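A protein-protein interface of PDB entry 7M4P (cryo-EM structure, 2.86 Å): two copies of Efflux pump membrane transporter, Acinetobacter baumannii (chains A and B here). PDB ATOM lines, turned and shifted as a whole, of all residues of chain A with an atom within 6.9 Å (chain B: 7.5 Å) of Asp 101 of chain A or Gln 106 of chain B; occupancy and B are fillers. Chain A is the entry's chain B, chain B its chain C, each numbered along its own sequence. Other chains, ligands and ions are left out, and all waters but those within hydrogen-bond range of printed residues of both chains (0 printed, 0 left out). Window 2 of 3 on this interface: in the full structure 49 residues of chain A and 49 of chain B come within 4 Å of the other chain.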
ATOM      1  N   VAL A  98     -27.896   2.595  22.005  1.00  0.00           N
ATOM      2  CA  VAL A  98     -26.683   1.893  21.635  1.00  0.00           C
ATOM      3  C   VAL A  98     -26.310   2.295  20.217  1.00  0.00           C
ATOM      4  O   VAL A  98     -27.174   2.431  19.345  1.00  0.00           O
ATOM      5  CB  VAL A  98     -26.873   0.371  21.770  1.00  0.00           C
ATOM      6  CG1 VAL A  98     -25.707  -0.378  21.179  1.00  0.00           C
ATOM      7  CG2 VAL A  98     -27.049  -0.013  23.214  1.00  0.00           C
ATOM      8  N   ASP A  99     -25.029   2.524  19.988  1.00  0.00           N
ATOM      9  CA  ASP A  99     -24.575   2.869  18.651  1.00  0.00           C
ATOM     10  C   ASP A  99     -24.616   1.616  17.785  1.00  0.00           C
ATOM     11  O   ASP A  99     -23.892   0.661  18.075  1.00  0.00           O
ATOM     12  CB  ASP A  99     -23.163   3.445  18.709  1.00  0.00           C
ATOM     13  CG  ASP A  99     -22.617   3.803  17.344  1.00  0.00           C
ATOM     14  OD1 ASP A  99     -23.397   3.859  16.375  1.00  0.00           O
ATOM     15  OD2 ASP A  99     -21.404   4.033  17.232  1.00  0.00           O
ATOM     16  N   PRO A 100     -25.437   1.568  16.736  1.00  0.00           N
ATOM     17  CA  PRO A 100     -25.568   0.314  15.978  1.00  0.00           C
ATOM     18  C   PRO A 100     -24.276  -0.172  15.343  1.00  0.00           C
ATOM     19  O   PRO A 100     -24.044  -1.385  15.291  1.00  0.00           O
ATOM     20  CB  PRO A 100     -26.638   0.653  14.933  1.00  0.00           C
ATOM     21  CG  PRO A 100     -26.749   2.093  14.922  1.00  0.00           C
ATOM     22  CD  PRO A 100     -26.368   2.591  16.251  1.00  0.00           C
ATOM     23  N   ASP A 101     -23.421   0.737  14.875  1.00  0.00           N
ATOM     24  CA  ASP A 101     -22.141   0.329  14.301  1.00  0.00           C
ATOM     25  C   ASP A 101     -21.237  -0.314  15.345  1.00  0.00           C
ATOM     26  O   ASP A 101     -20.575  -1.322  15.072  1.00  0.00           O
ATOM     27  CB  ASP A 101     -21.453   1.536  13.669  1.00  0.00           C
ATOM     28  CG  ASP A 101     -21.727   1.645  12.182  1.00  0.00           C
ATOM     29  OD1 ASP A 101     -21.439   0.682  11.448  1.00  0.00           O
ATOM     30  OD2 ASP A 101     -22.256   2.687  11.752  1.00  0.00           O
ATOM     31  N   ILE A 102     -21.197   0.259  16.543  1.00  0.00           N
ATOM     32  CA  ILE A 102     -20.380  -0.286  17.613  1.00  0.00           C
ATOM     33  C   ILE A 102     -20.903  -1.647  18.047  1.00  0.00           C
ATOM     34  O   ILE A 102     -20.129  -2.593  18.232  1.00  0.00           O
ATOM     35  CB  ILE A 102     -20.327   0.721  18.774  1.00  0.00           C
ATOM     36  CG1 ILE A 102     -19.565   1.969  18.326  1.00  0.00           C
ATOM     37  CG2 ILE A 102     -19.714   0.093  20.011  1.00  0.00           C
ATOM     38  CD1 ILE A 102     -18.098   1.766  18.082  1.00  0.00           C
ATOM     39  N   ALA A 103     -22.223  -1.774  18.192  1.00  0.00           N
ATOM     40  CA  ALA A 103     -22.820  -3.061  18.522  1.00  0.00           C
ATOM     41  C   ALA A 103     -22.475  -4.113  17.476  1.00  0.00           C
ATOM     42  O   ALA A 103     -22.133  -5.252  17.820  1.00  0.00           O
ATOM     43  CB  ALA A 103     -24.331  -2.906  18.664  1.00  0.00           C
ATOM     44  N   GLN A 104     -22.530  -3.747  16.194  1.00  0.00           N
ATOM     45  CA  GLN A 104     -22.245  -4.719  15.142  1.00  0.00           C
ATOM     46  C   GLN A 104     -20.791  -5.175  15.178  1.00  0.00           C
ATOM     47  O   GLN A 104     -20.505  -6.376  15.068  1.00  0.00           O
ATOM     48  CB  GLN A 104     -22.593  -4.138  13.773  1.00  0.00           C
ATOM     49  CG  GLN A 104     -22.969  -5.206  12.753  1.00  0.00           C
ATOM     50  CD  GLN A 104     -22.609  -4.864  11.329  1.00  0.00           C
ATOM     51  OE1 GLN A 104     -23.032  -3.852  10.797  1.00  0.00           O
ATOM     52  NE2 GLN A 104     -21.848  -5.729  10.699  1.00  0.00           N
ATOM     53  N   VAL A 105     -19.850  -4.234  15.320  1.00  0.00           N
ATOM     54  CA  VAL A 105     -18.445  -4.636  15.360  1.00  0.00           C
ATOM     55  C   VAL A 105     -18.174  -5.502  16.574  1.00  0.00           C
ATOM     56  O   VAL A 105     -17.430  -6.480  16.492  1.00  0.00           O
ATOM     57  CB  VAL A 105     -17.481  -3.433  15.323  1.00  0.00           C
ATOM     58  CG1 VAL A 105     -17.525  -2.764  13.991  1.00  0.00           C
ATOM     59  CG2 VAL A 105     -17.761  -2.446  16.429  1.00  0.00           C
ATOM     60  N   GLN A 106     -18.758  -5.162  17.724  1.00  0.00           N
ATOM     61  CA  GLN A 106     -18.543  -5.986  18.905  1.00  0.00           C
ATOM     62  C   GLN A 106     -19.050  -7.408  18.692  1.00  0.00           C
ATOM     63  O   GLN A 106     -18.372  -8.378  19.058  1.00  0.00           O
ATOM     64  CB  GLN A 106     -19.208  -5.348  20.118  1.00  0.00           C
ATOM     65  CG  GLN A 106     -18.558  -4.061  20.553  1.00  0.00           C
ATOM     66  CD  GLN A 106     -19.173  -3.454  21.791  1.00  0.00           C
ATOM     67  OE1 GLN A 106     -20.230  -3.871  22.244  1.00  0.00           O
ATOM     68  NE2 GLN A 106     -18.513  -2.459  22.342  1.00  0.00           N
ATOM     69  N   GLN A 108     -19.409  -9.140  15.840  1.00  0.00           N
ATOM     70  CA  GLN A 108     -18.608  -9.935  14.934  1.00  0.00           C
ATOM     71  C   GLN A 108     -17.233 -10.208  15.487  1.00  0.00           C
ATOM     72  O   GLN A 108     -16.606 -11.176  15.113  1.00  0.00           O
ATOM     73  CB  GLN A 108     -18.551  -9.358  13.529  1.00  0.00           C
ATOM     74  CG  GLN A 108     -17.877  -8.039  13.419  1.00  0.00           C
ATOM     75  CD  GLN A 108     -18.256  -7.317  12.164  1.00  0.00           C
ATOM     76  OE1 GLN A 108     -19.415  -7.200  11.841  1.00  0.00           O
ATOM     77  NE2 GLN A 108     -17.283  -6.825  11.454  1.00  0.00           N
ATOM     78  N   LYS A 131     -26.530  -5.571  10.631  1.00  0.00           N
ATOM     79  CA  LYS A 131     -27.399  -4.830  11.533  1.00  0.00           C
ATOM     80  C   LYS A 131     -28.659  -4.396  10.802  1.00  0.00           C
ATOM     81  O   LYS A 131     -28.741  -4.455   9.577  1.00  0.00           O
ATOM     82  CB  LYS A 131     -26.696  -3.605  12.126  1.00  0.00           C
ATOM     83  CG  LYS A 131     -26.032  -2.724  11.115  1.00  0.00           C
ATOM     84  CD  LYS A 131     -25.573  -1.432  11.720  1.00  0.00           C
ATOM     85  CE  LYS A 131     -24.563  -0.768  10.842  1.00  0.00           C
ATOM     86  NZ  LYS A 131     -24.440   0.668  11.178  1.00  0.00           N
ATOM     87  N   MET B  69     -18.388  -1.289  -0.487  1.00  0.00           N
ATOM     88  CA  MET B  69     -18.077  -0.013   0.110  1.00  0.00           C
ATOM     89  C   MET B  69     -18.912   1.164  -0.407  1.00  0.00           C
ATOM     90  O   MET B  69     -18.944   2.210   0.212  1.00  0.00           O
ATOM     91  CB  MET B  69     -16.598   0.289  -0.073  1.00  0.00           C
ATOM     92  CG  MET B  69     -15.653  -0.700   0.572  1.00  0.00           C
ATOM     93  SD  MET B  69     -15.913  -1.002   2.319  1.00  0.00           S
ATOM     94  CE  MET B  69     -16.388  -2.713   2.379  1.00  0.00           C
ATOM     95  N   GLY B  71     -21.528   3.386  -0.339  1.00  0.00           N
ATOM     96  CA  GLY B  71     -22.569   3.606   0.644  1.00  0.00           C
ATOM     97  C   GLY B  71     -22.044   3.764   2.051  1.00  0.00           C
ATOM     98  O   GLY B  71     -22.795   3.627   3.015  1.00  0.00           O
ATOM     99  N   LEU B  72     -20.752   4.021   2.185  1.00  0.00           N
ATOM    100  CA  LEU B  72     -20.223   4.518   3.439  1.00  0.00           C
ATOM    101  C   LEU B  72     -20.650   5.969   3.635  1.00  0.00           C
ATOM    102  O   LEU B  72     -20.999   6.673   2.689  1.00  0.00           O
ATOM    103  CB  LEU B  72     -18.705   4.380   3.460  1.00  0.00           C
ATOM    104  CG  LEU B  72     -18.220   2.928   3.419  1.00  0.00           C
ATOM    105  CD1 LEU B  72     -16.753   2.850   3.067  1.00  0.00           C
ATOM    106  CD2 LEU B  72     -18.483   2.250   4.746  1.00  0.00           C
ATOM    107  N   ASP B  73     -20.624   6.409   4.893  1.00  0.00           N
ATOM    108  CA  ASP B  73     -21.237   7.663   5.301  1.00  0.00           C
ATOM    109  C   ASP B  73     -20.699   8.883   4.567  1.00  0.00           C
ATOM    110  O   ASP B  73     -21.431   9.536   3.817  1.00  0.00           O
ATOM    111  CB  ASP B  73     -21.051   7.865   6.803  1.00  0.00           C
ATOM    112  CG  ASP B  73     -21.770   9.097   7.322  1.00  0.00           C
ATOM    113  OD1 ASP B  73     -22.685   9.596   6.634  1.00  0.00           O
ATOM    114  OD2 ASP B  73     -21.408   9.572   8.418  1.00  0.00           O
ATOM    115  N   GLY B  74     -19.426   9.190   4.754  1.00  0.00           N
ATOM    116  CA  GLY B  74     -18.882  10.447   4.292  1.00  0.00           C
ATOM    117  C   GLY B  74     -17.812  10.201   3.262  1.00  0.00           C
ATOM    118  O   GLY B  74     -16.769  10.852   3.255  1.00  0.00           O
ATOM    119  N   LEU B  92     -10.026   4.088   0.415  1.00  0.00           N
ATOM    120  CA  LEU B  92     -11.235   4.866   0.561  1.00  0.00           C
ATOM    121  C   LEU B  92     -10.946   6.215   1.174  1.00  0.00           C
ATOM    122  O   LEU B  92     -10.413   6.293   2.254  1.00  0.00           O
ATOM    123  CB  LEU B  92     -12.205   4.128   1.483  1.00  0.00           C
ATOM    124  CG  LEU B  92     -12.420   2.640   1.242  1.00  0.00           C
ATOM    125  CD1 LEU B  92     -12.961   1.974   2.478  1.00  0.00           C
ATOM    126  CD2 LEU B  92     -13.343   2.409   0.075  1.00  0.00           C
ATOM    127  N   PHE B  94     -12.311   9.959   2.589  1.00  0.00           N
ATOM    128  CA  PHE B  94     -13.493  10.429   3.280  1.00  0.00           C
ATOM    129  C   PHE B  94     -13.523  11.942   3.299  1.00  0.00           C
ATOM    130  O   PHE B  94     -12.522  12.610   3.056  1.00  0.00           O
ATOM    131  CB  PHE B  94     -13.542   9.898   4.706  1.00  0.00           C
ATOM    132  CG  PHE B  94     -14.053   8.510   4.806  1.00  0.00           C
ATOM    133  CD1 PHE B  94     -15.401   8.271   4.915  1.00  0.00           C
ATOM    134  CD2 PHE B  94     -13.193   7.441   4.769  1.00  0.00           C
ATOM    135  CE1 PHE B  94     -15.875   7.002   5.003  1.00  0.00           C
ATOM    136  CE2 PHE B  94     -13.663   6.170   4.852  1.00  0.00           C
ATOM    137  CZ  PHE B  94     -15.004   5.947   4.975  1.00  0.00           C
ATOM    138  N   VAL B  98     -15.077  13.657   9.033  1.00  0.00           N
ATOM    139  CA  VAL B  98     -15.454  12.283   9.333  1.00  0.00           C
ATOM    140  C   VAL B  98     -14.454  11.734  10.337  1.00  0.00           C
ATOM    141  O   VAL B  98     -13.249  11.946  10.196  1.00  0.00           O
ATOM    142  CB  VAL B  98     -15.495  11.444   8.041  1.00  0.00           C
ATOM    143  CG1 VAL B  98     -15.815   9.988   8.317  1.00  0.00           C
ATOM    144  CG2 VAL B  98     -16.488  12.032   7.071  1.00  0.00           C
ATOM    145  N   ASP B  99     -14.940  11.062  11.359  1.00  0.00           N
ATOM    146  CA  ASP B  99     -14.057  10.556  12.408  1.00  0.00           C
ATOM    147  C   ASP B  99     -13.329   9.306  11.926  1.00  0.00           C
ATOM    148  O   ASP B  99     -13.977   8.351  11.493  1.00  0.00           O
ATOM    149  CB  ASP B  99     -14.846  10.237  13.665  1.00  0.00           C
ATOM    150  CG  ASP B  99     -14.002   9.608  14.735  1.00  0.00           C
ATOM    151  OD1 ASP B  99     -12.762   9.667  14.640  1.00  0.00           O
ATOM    152  OD2 ASP B  99     -14.579   9.057  15.688  1.00  0.00           O
ATOM    153  N   PRO B 100     -11.994   9.272  11.989  1.00  0.00           N
ATOM    154  CA  PRO B 100     -11.269   8.095  11.485  1.00  0.00           C
ATOM    155  C   PRO B 100     -11.683   6.777  12.116  1.00  0.00           C
ATOM    156  O   PRO B 100     -11.776   5.763  11.417  1.00  0.00           O
ATOM    157  CB  PRO B 100      -9.817   8.441  11.811  1.00  0.00           C
ATOM    158  CG  PRO B 100      -9.776   9.894  11.735  1.00  0.00           C
ATOM    159  CD  PRO B 100     -11.078  10.389  12.253  1.00  0.00           C
ATOM    160  N   ASP B 101     -11.940   6.758  13.420  1.00  0.00           N
ATOM    161  CA  ASP B 101     -12.270   5.500  14.076  1.00  0.00           C
ATOM    162  C   ASP B 101     -13.646   5.002  13.657  1.00  0.00           C
ATOM    163  O   ASP B 101     -13.848   3.796  13.450  1.00  0.00           O
ATOM    164  CB  ASP B 101     -12.179   5.684  15.582  1.00  0.00           C
ATOM    165  CG  ASP B 101     -10.768   5.939  16.041  1.00  0.00           C
ATOM    166  OD1 ASP B 101      -9.830   5.519  15.341  1.00  0.00           O
ATOM    167  OD2 ASP B 101     -10.588   6.557  17.106  1.00  0.00           O
ATOM    168  N   ILE B 102     -14.599   5.916  13.496  1.00  0.00           N
ATOM    169  CA  ILE B 102     -15.912   5.528  13.005  1.00  0.00           C
ATOM    170  C   ILE B 102     -15.815   5.014  11.579  1.00  0.00           C
ATOM    171  O   ILE B 102     -16.456   4.024  11.219  1.00  0.00           O
ATOM    172  CB  ILE B 102     -16.894   6.702  13.129  1.00  0.00           C
ATOM    173  CG1 ILE B 102     -16.957   7.177  14.578  1.00  0.00           C
ATOM    174  CG2 ILE B 102     -18.258   6.293  12.643  1.00  0.00           C
ATOM    175  CD1 ILE B 102     -16.805   6.085  15.615  1.00  0.00           C
ATOM    176  N   ALA B 103     -15.008   5.669  10.747  1.00  0.00           N
ATOM    177  CA  ALA B 103     -14.820   5.187   9.385  1.00  0.00           C
ATOM    178  C   ALA B 103     -14.228   3.784   9.376  1.00  0.00           C
ATOM    179  O   ALA B 103     -14.672   2.928   8.607  1.00  0.00           O
ATOM    180  CB  ALA B 103     -13.930   6.150   8.601  1.00  0.00           C
ATOM    181  N   GLN B 104     -13.228   3.526  10.219  1.00  0.00           N
ATOM    182  CA  GLN B 104     -12.609   2.203  10.236  1.00  0.00           C
ATOM    183  C   GLN B 104     -13.606   1.132  10.659  1.00  0.00           C
ATOM    184  O   GLN B 104     -13.688   0.064  10.035  1.00  0.00           O
ATOM    185  CB  GLN B 104     -11.398   2.189  11.165  1.00  0.00           C
ATOM    186  CG  GLN B 104     -10.463   1.042  10.878  1.00  0.00           C
ATOM    187  CD  GLN B 104      -9.677   0.597  12.078  1.00  0.00           C
ATOM    188  OE1 GLN B 104      -9.444  -0.592  12.266  1.00  0.00           O
ATOM    189  NE2 GLN B 104      -9.237   1.546  12.889  1.00  0.00           N
ATOM    190  N   VAL B 105     -14.379   1.400  11.718  1.00  0.00           N
ATOM    191  CA  VAL B 105     -15.329   0.399  12.190  1.00  0.00           C
ATOM    192  C   VAL B 105     -16.403   0.152  11.142  1.00  0.00           C
ATOM    193  O   VAL B 105     -16.836  -0.984  10.939  1.00  0.00           O
ATOM    194  CB  VAL B 105     -15.949   0.801  13.546  1.00  0.00           C
ATOM    195  CG1 VAL B 105     -14.901   0.866  14.612  1.00  0.00           C
ATOM    196  CG2 VAL B 105     -16.670   2.112  13.445  1.00  0.00           C
ATOM    197  N   GLN B 106     -16.841   1.202  10.454  1.00  0.00           N
ATOM    198  CA  GLN B 106     -17.847   1.025   9.417  1.00  0.00           C
ATOM    199  C   GLN B 106     -17.310   0.211   8.250  1.00  0.00           C
ATOM    200  O   GLN B 106     -18.028  -0.620   7.675  1.00  0.00           O
ATOM    201  CB  GLN B 106     -18.336   2.384   8.948  1.00  0.00           C
ATOM    202  CG  GLN B 106     -19.189   3.095   9.951  1.00  0.00           C
ATOM    203  CD  GLN B 106     -19.962   4.227   9.339  1.00  0.00           C
ATOM    204  OE1 GLN B 106     -20.333   4.178   8.172  1.00  0.00           O
ATOM    205  NE2 GLN B 106     -20.212   5.257  10.122  1.00  0.00           N
ATOM    206  N   VAL B 107     -16.056   0.445   7.881  1.00  0.00           N
ATOM    207  CA  VAL B 107     -15.456  -0.301   6.786  1.00  0.00           C
ATOM    208  C   VAL B 107     -15.378  -1.770   7.143  1.00  0.00           C
ATOM    209  O   VAL B 107     -15.659  -2.639   6.314  1.00  0.00           O
ATOM    210  CB  VAL B 107     -14.074   0.283   6.451  1.00  0.00           C
ATOM    211  CG1 VAL B 107     -13.387  -0.550   5.414  1.00  0.00           C
ATOM    212  CG2 VAL B 107     -14.216   1.699   5.974  1.00  0.00           C
ATOM    213  N   GLN B 108     -14.999  -2.074   8.385  1.00  0.00           N
ATOM    214  CA  GLN B 108     -15.007  -3.461   8.831  1.00  0.00           C
ATOM    215  C   GLN B 108     -16.415  -4.044   8.810  1.00  0.00           C
ATOM    216  O   GLN B 108     -16.609  -5.202   8.426  1.00  0.00           O
ATOM    217  CB  GLN B 108     -14.406  -3.552  10.227  1.00  0.00           C
ATOM    218  CG  GLN B 108     -12.927  -3.244  10.251  1.00  0.00           C
ATOM    219  CD  GLN B 108     -12.355  -3.195  11.644  1.00  0.00           C
ATOM    220  OE1 GLN B 108     -11.568  -2.314  11.966  1.00  0.00           O
ATOM    221  NE2 GLN B 108     -12.732  -4.152  12.474  1.00  0.00           N
ATOM    222  N   ASN B 109     -17.409  -3.262   9.227  1.00  0.00           N
ATOM    223  CA  ASN B 109     -18.774  -3.770   9.269  1.00  0.00           C
ATOM    224  C   ASN B 109     -19.259  -4.179   7.888  1.00  0.00           C
ATOM    225  O   ASN B 109     -19.950  -5.191   7.742  1.00  0.00           O
ATOM    226  CB  ASN B 109     -19.702  -2.729   9.874  1.00  0.00           C
ATOM    227  CG  ASN B 109     -19.690  -2.751  11.377  1.00  0.00           C
ATOM    228  OD1 ASN B 109     -19.257  -3.714  11.986  1.00  0.00           O
ATOM    229  ND2 ASN B 109     -20.188  -1.696  11.983  1.00  0.00           N
ATOM    230  N   LYS B 110     -18.922  -3.404   6.859  1.00  0.00           N
ATOM    231  CA  LYS B 110     -19.292  -3.812   5.503  1.00  0.00           C
ATOM    232  C   LYS B 110     -18.417  -4.960   5.001  1.00  0.00           C
ATOM    233  O   LYS B 110     -18.901  -5.878   4.314  1.00  0.00           O
ATOM    234  CB  LYS B 110     -19.211  -2.618   4.558  1.00  0.00           C
ATOM    235  CG  LYS B 110     -20.450  -1.758   4.572  1.00  0.00           C
ATOM    236  CD  LYS B 110     -20.373  -0.682   3.531  1.00  0.00           C
ATOM    237  CE  LYS B 110     -21.716  -0.003   3.304  1.00  0.00           C
ATOM    238  NZ  LYS B 110     -21.839   0.552   1.921  1.00  0.00           N
ATOM    239  N   LEU B 111     -17.129  -4.934   5.335  1.00  0.00           N
ATOM    240  CA  LEU B 111     -16.225  -5.967   4.861  1.00  0.00           C
ATOM    241  C   LEU B 111     -16.632  -7.339   5.364  1.00  0.00           C
ATOM    242  O   LEU B 111     -16.394  -8.344   4.690  1.00  0.00           O
ATOM    243  CB  LEU B 111     -14.805  -5.635   5.307  1.00  0.00           C
ATOM    244  CG  LEU B 111     -13.684  -6.371   4.587  1.00  0.00           C
ATOM    245  CD1 LEU B 111     -13.650  -5.955   3.140  1.00  0.00           C
ATOM    246  CD2 LEU B 111     -12.370  -6.092   5.267  1.00  0.00           C
ATOM    247  N   GLN B 112     -17.221  -7.399   6.555  1.00  0.00           N
ATOM    248  CA  GLN B 112     -17.623  -8.673   7.134  1.00  0.00           C
ATOM    249  C   GLN B 112     -18.497  -9.459   6.172  1.00  0.00           C
ATOM    250  O   GLN B 112     -18.227 -10.625   5.870  1.00  0.00           O
ATOM    251  CB  GLN B 112     -18.357  -8.404   8.446  1.00  0.00           C
ATOM    252  CG  GLN B 112     -19.260  -9.505   8.952  1.00  0.00           C
ATOM    253  CD  GLN B 112     -18.488 -10.643   9.523  1.00  0.00           C
ATOM    254  OE1 GLN B 112     -17.570 -10.442  10.316  1.00  0.00           O
ATOM    255  NE2 GLN B 112     -18.832 -11.852   9.116  1.00  0.00           N
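Asp 101 of chain A touches Gln 106 of chain B, but with the chains exchanged Gln 106 of chain A does not touch Asp 101 of chain B (11.1 Å).
Val 105 of chain B touches its own counterpart, Val 105 of chain A.
Gln 108 of chain A touches its own counterpart, Gln 108 of chain B.
Of the 8 pairs that touch across the chains among the printed residues, 2 have their exchanged pair printed and touching as well.
Among the printed residues, pairs that only touch across the chains: Gln 108 of chain A with Gln 108 of chain B, Gln 104 of chain A with Asn 109 of chain B, Gln 108 of chain A with Gln 112 of chain B, Asp 101 of chain A with Gln 106 of chain B and Val 105 of chain A with Val 105 of chain B.
Val 98 of chain A touches none of the printed residues of chain B.
Of chain B, only Gln 106 and Asn 109 come within 4 Å of Asp 101 of chain A.
Ile 102 of chain A touches none of the printed residues of chain B.
Of the printed residues of chain A, Val 105 of chain B touches Val 105.
Printed residues of chain A within 4 Å of Gln 108 of chain B: Gln 108.
Printed residues of chain A within 4 Å of Asn 109 of chain B: Asp 101 (2.7 Å), Gln 104 (3.5 Å), Val 105 (2.8 Å) and Gln 108 (3.5 Å).
Of the printed residues of chain A, Gln 112 of chain B touches Gln 108 (3.5 Å).
The nearest residue of chain A that does not touch Gln 106 of chain B is Val 105 of chain A (5.4 Å).
The nearest printed residue of chain A that does not touch Gln 108 of chain B is Val 105 of chain A (5.0 Å).
OD1 of Asp 99 of chain A lies close to N of Asp 101 of chain A (3.5 Å).
OD1 of Asp 101 of chain A lies within salt-bridge range of NZ of Lys 131 of chain A, at 3.0 Å.
The side-chain amide nitrogen (NE2) of Gln 104 of chain A is in hydrogen-bond range of the side-chain amide oxygen (OE1) of Gln 108 of chain A (3.1 Å).
The side-chain amide oxygen (OE1) of Gln 104 of chain B sits close to the side-chain amide oxygen (OE1) of Gln 108 of chain B, 2.8 Å away.
The side-chain carboxylate of Asp 101 of chain A is in hydrogen-bond range of the side-chain amide nitrogen of Asn 109 of chain B, at 2.7 Å.
OD1 of Asn 109 of chain B lies close to N of Val 105 of chain A.
The side-chain amide oxygen (OD1) of Asn 109 of chain B lies close to the side-chain amide oxygen (OE1) of Gln 108 of chain A (3.5 Å).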
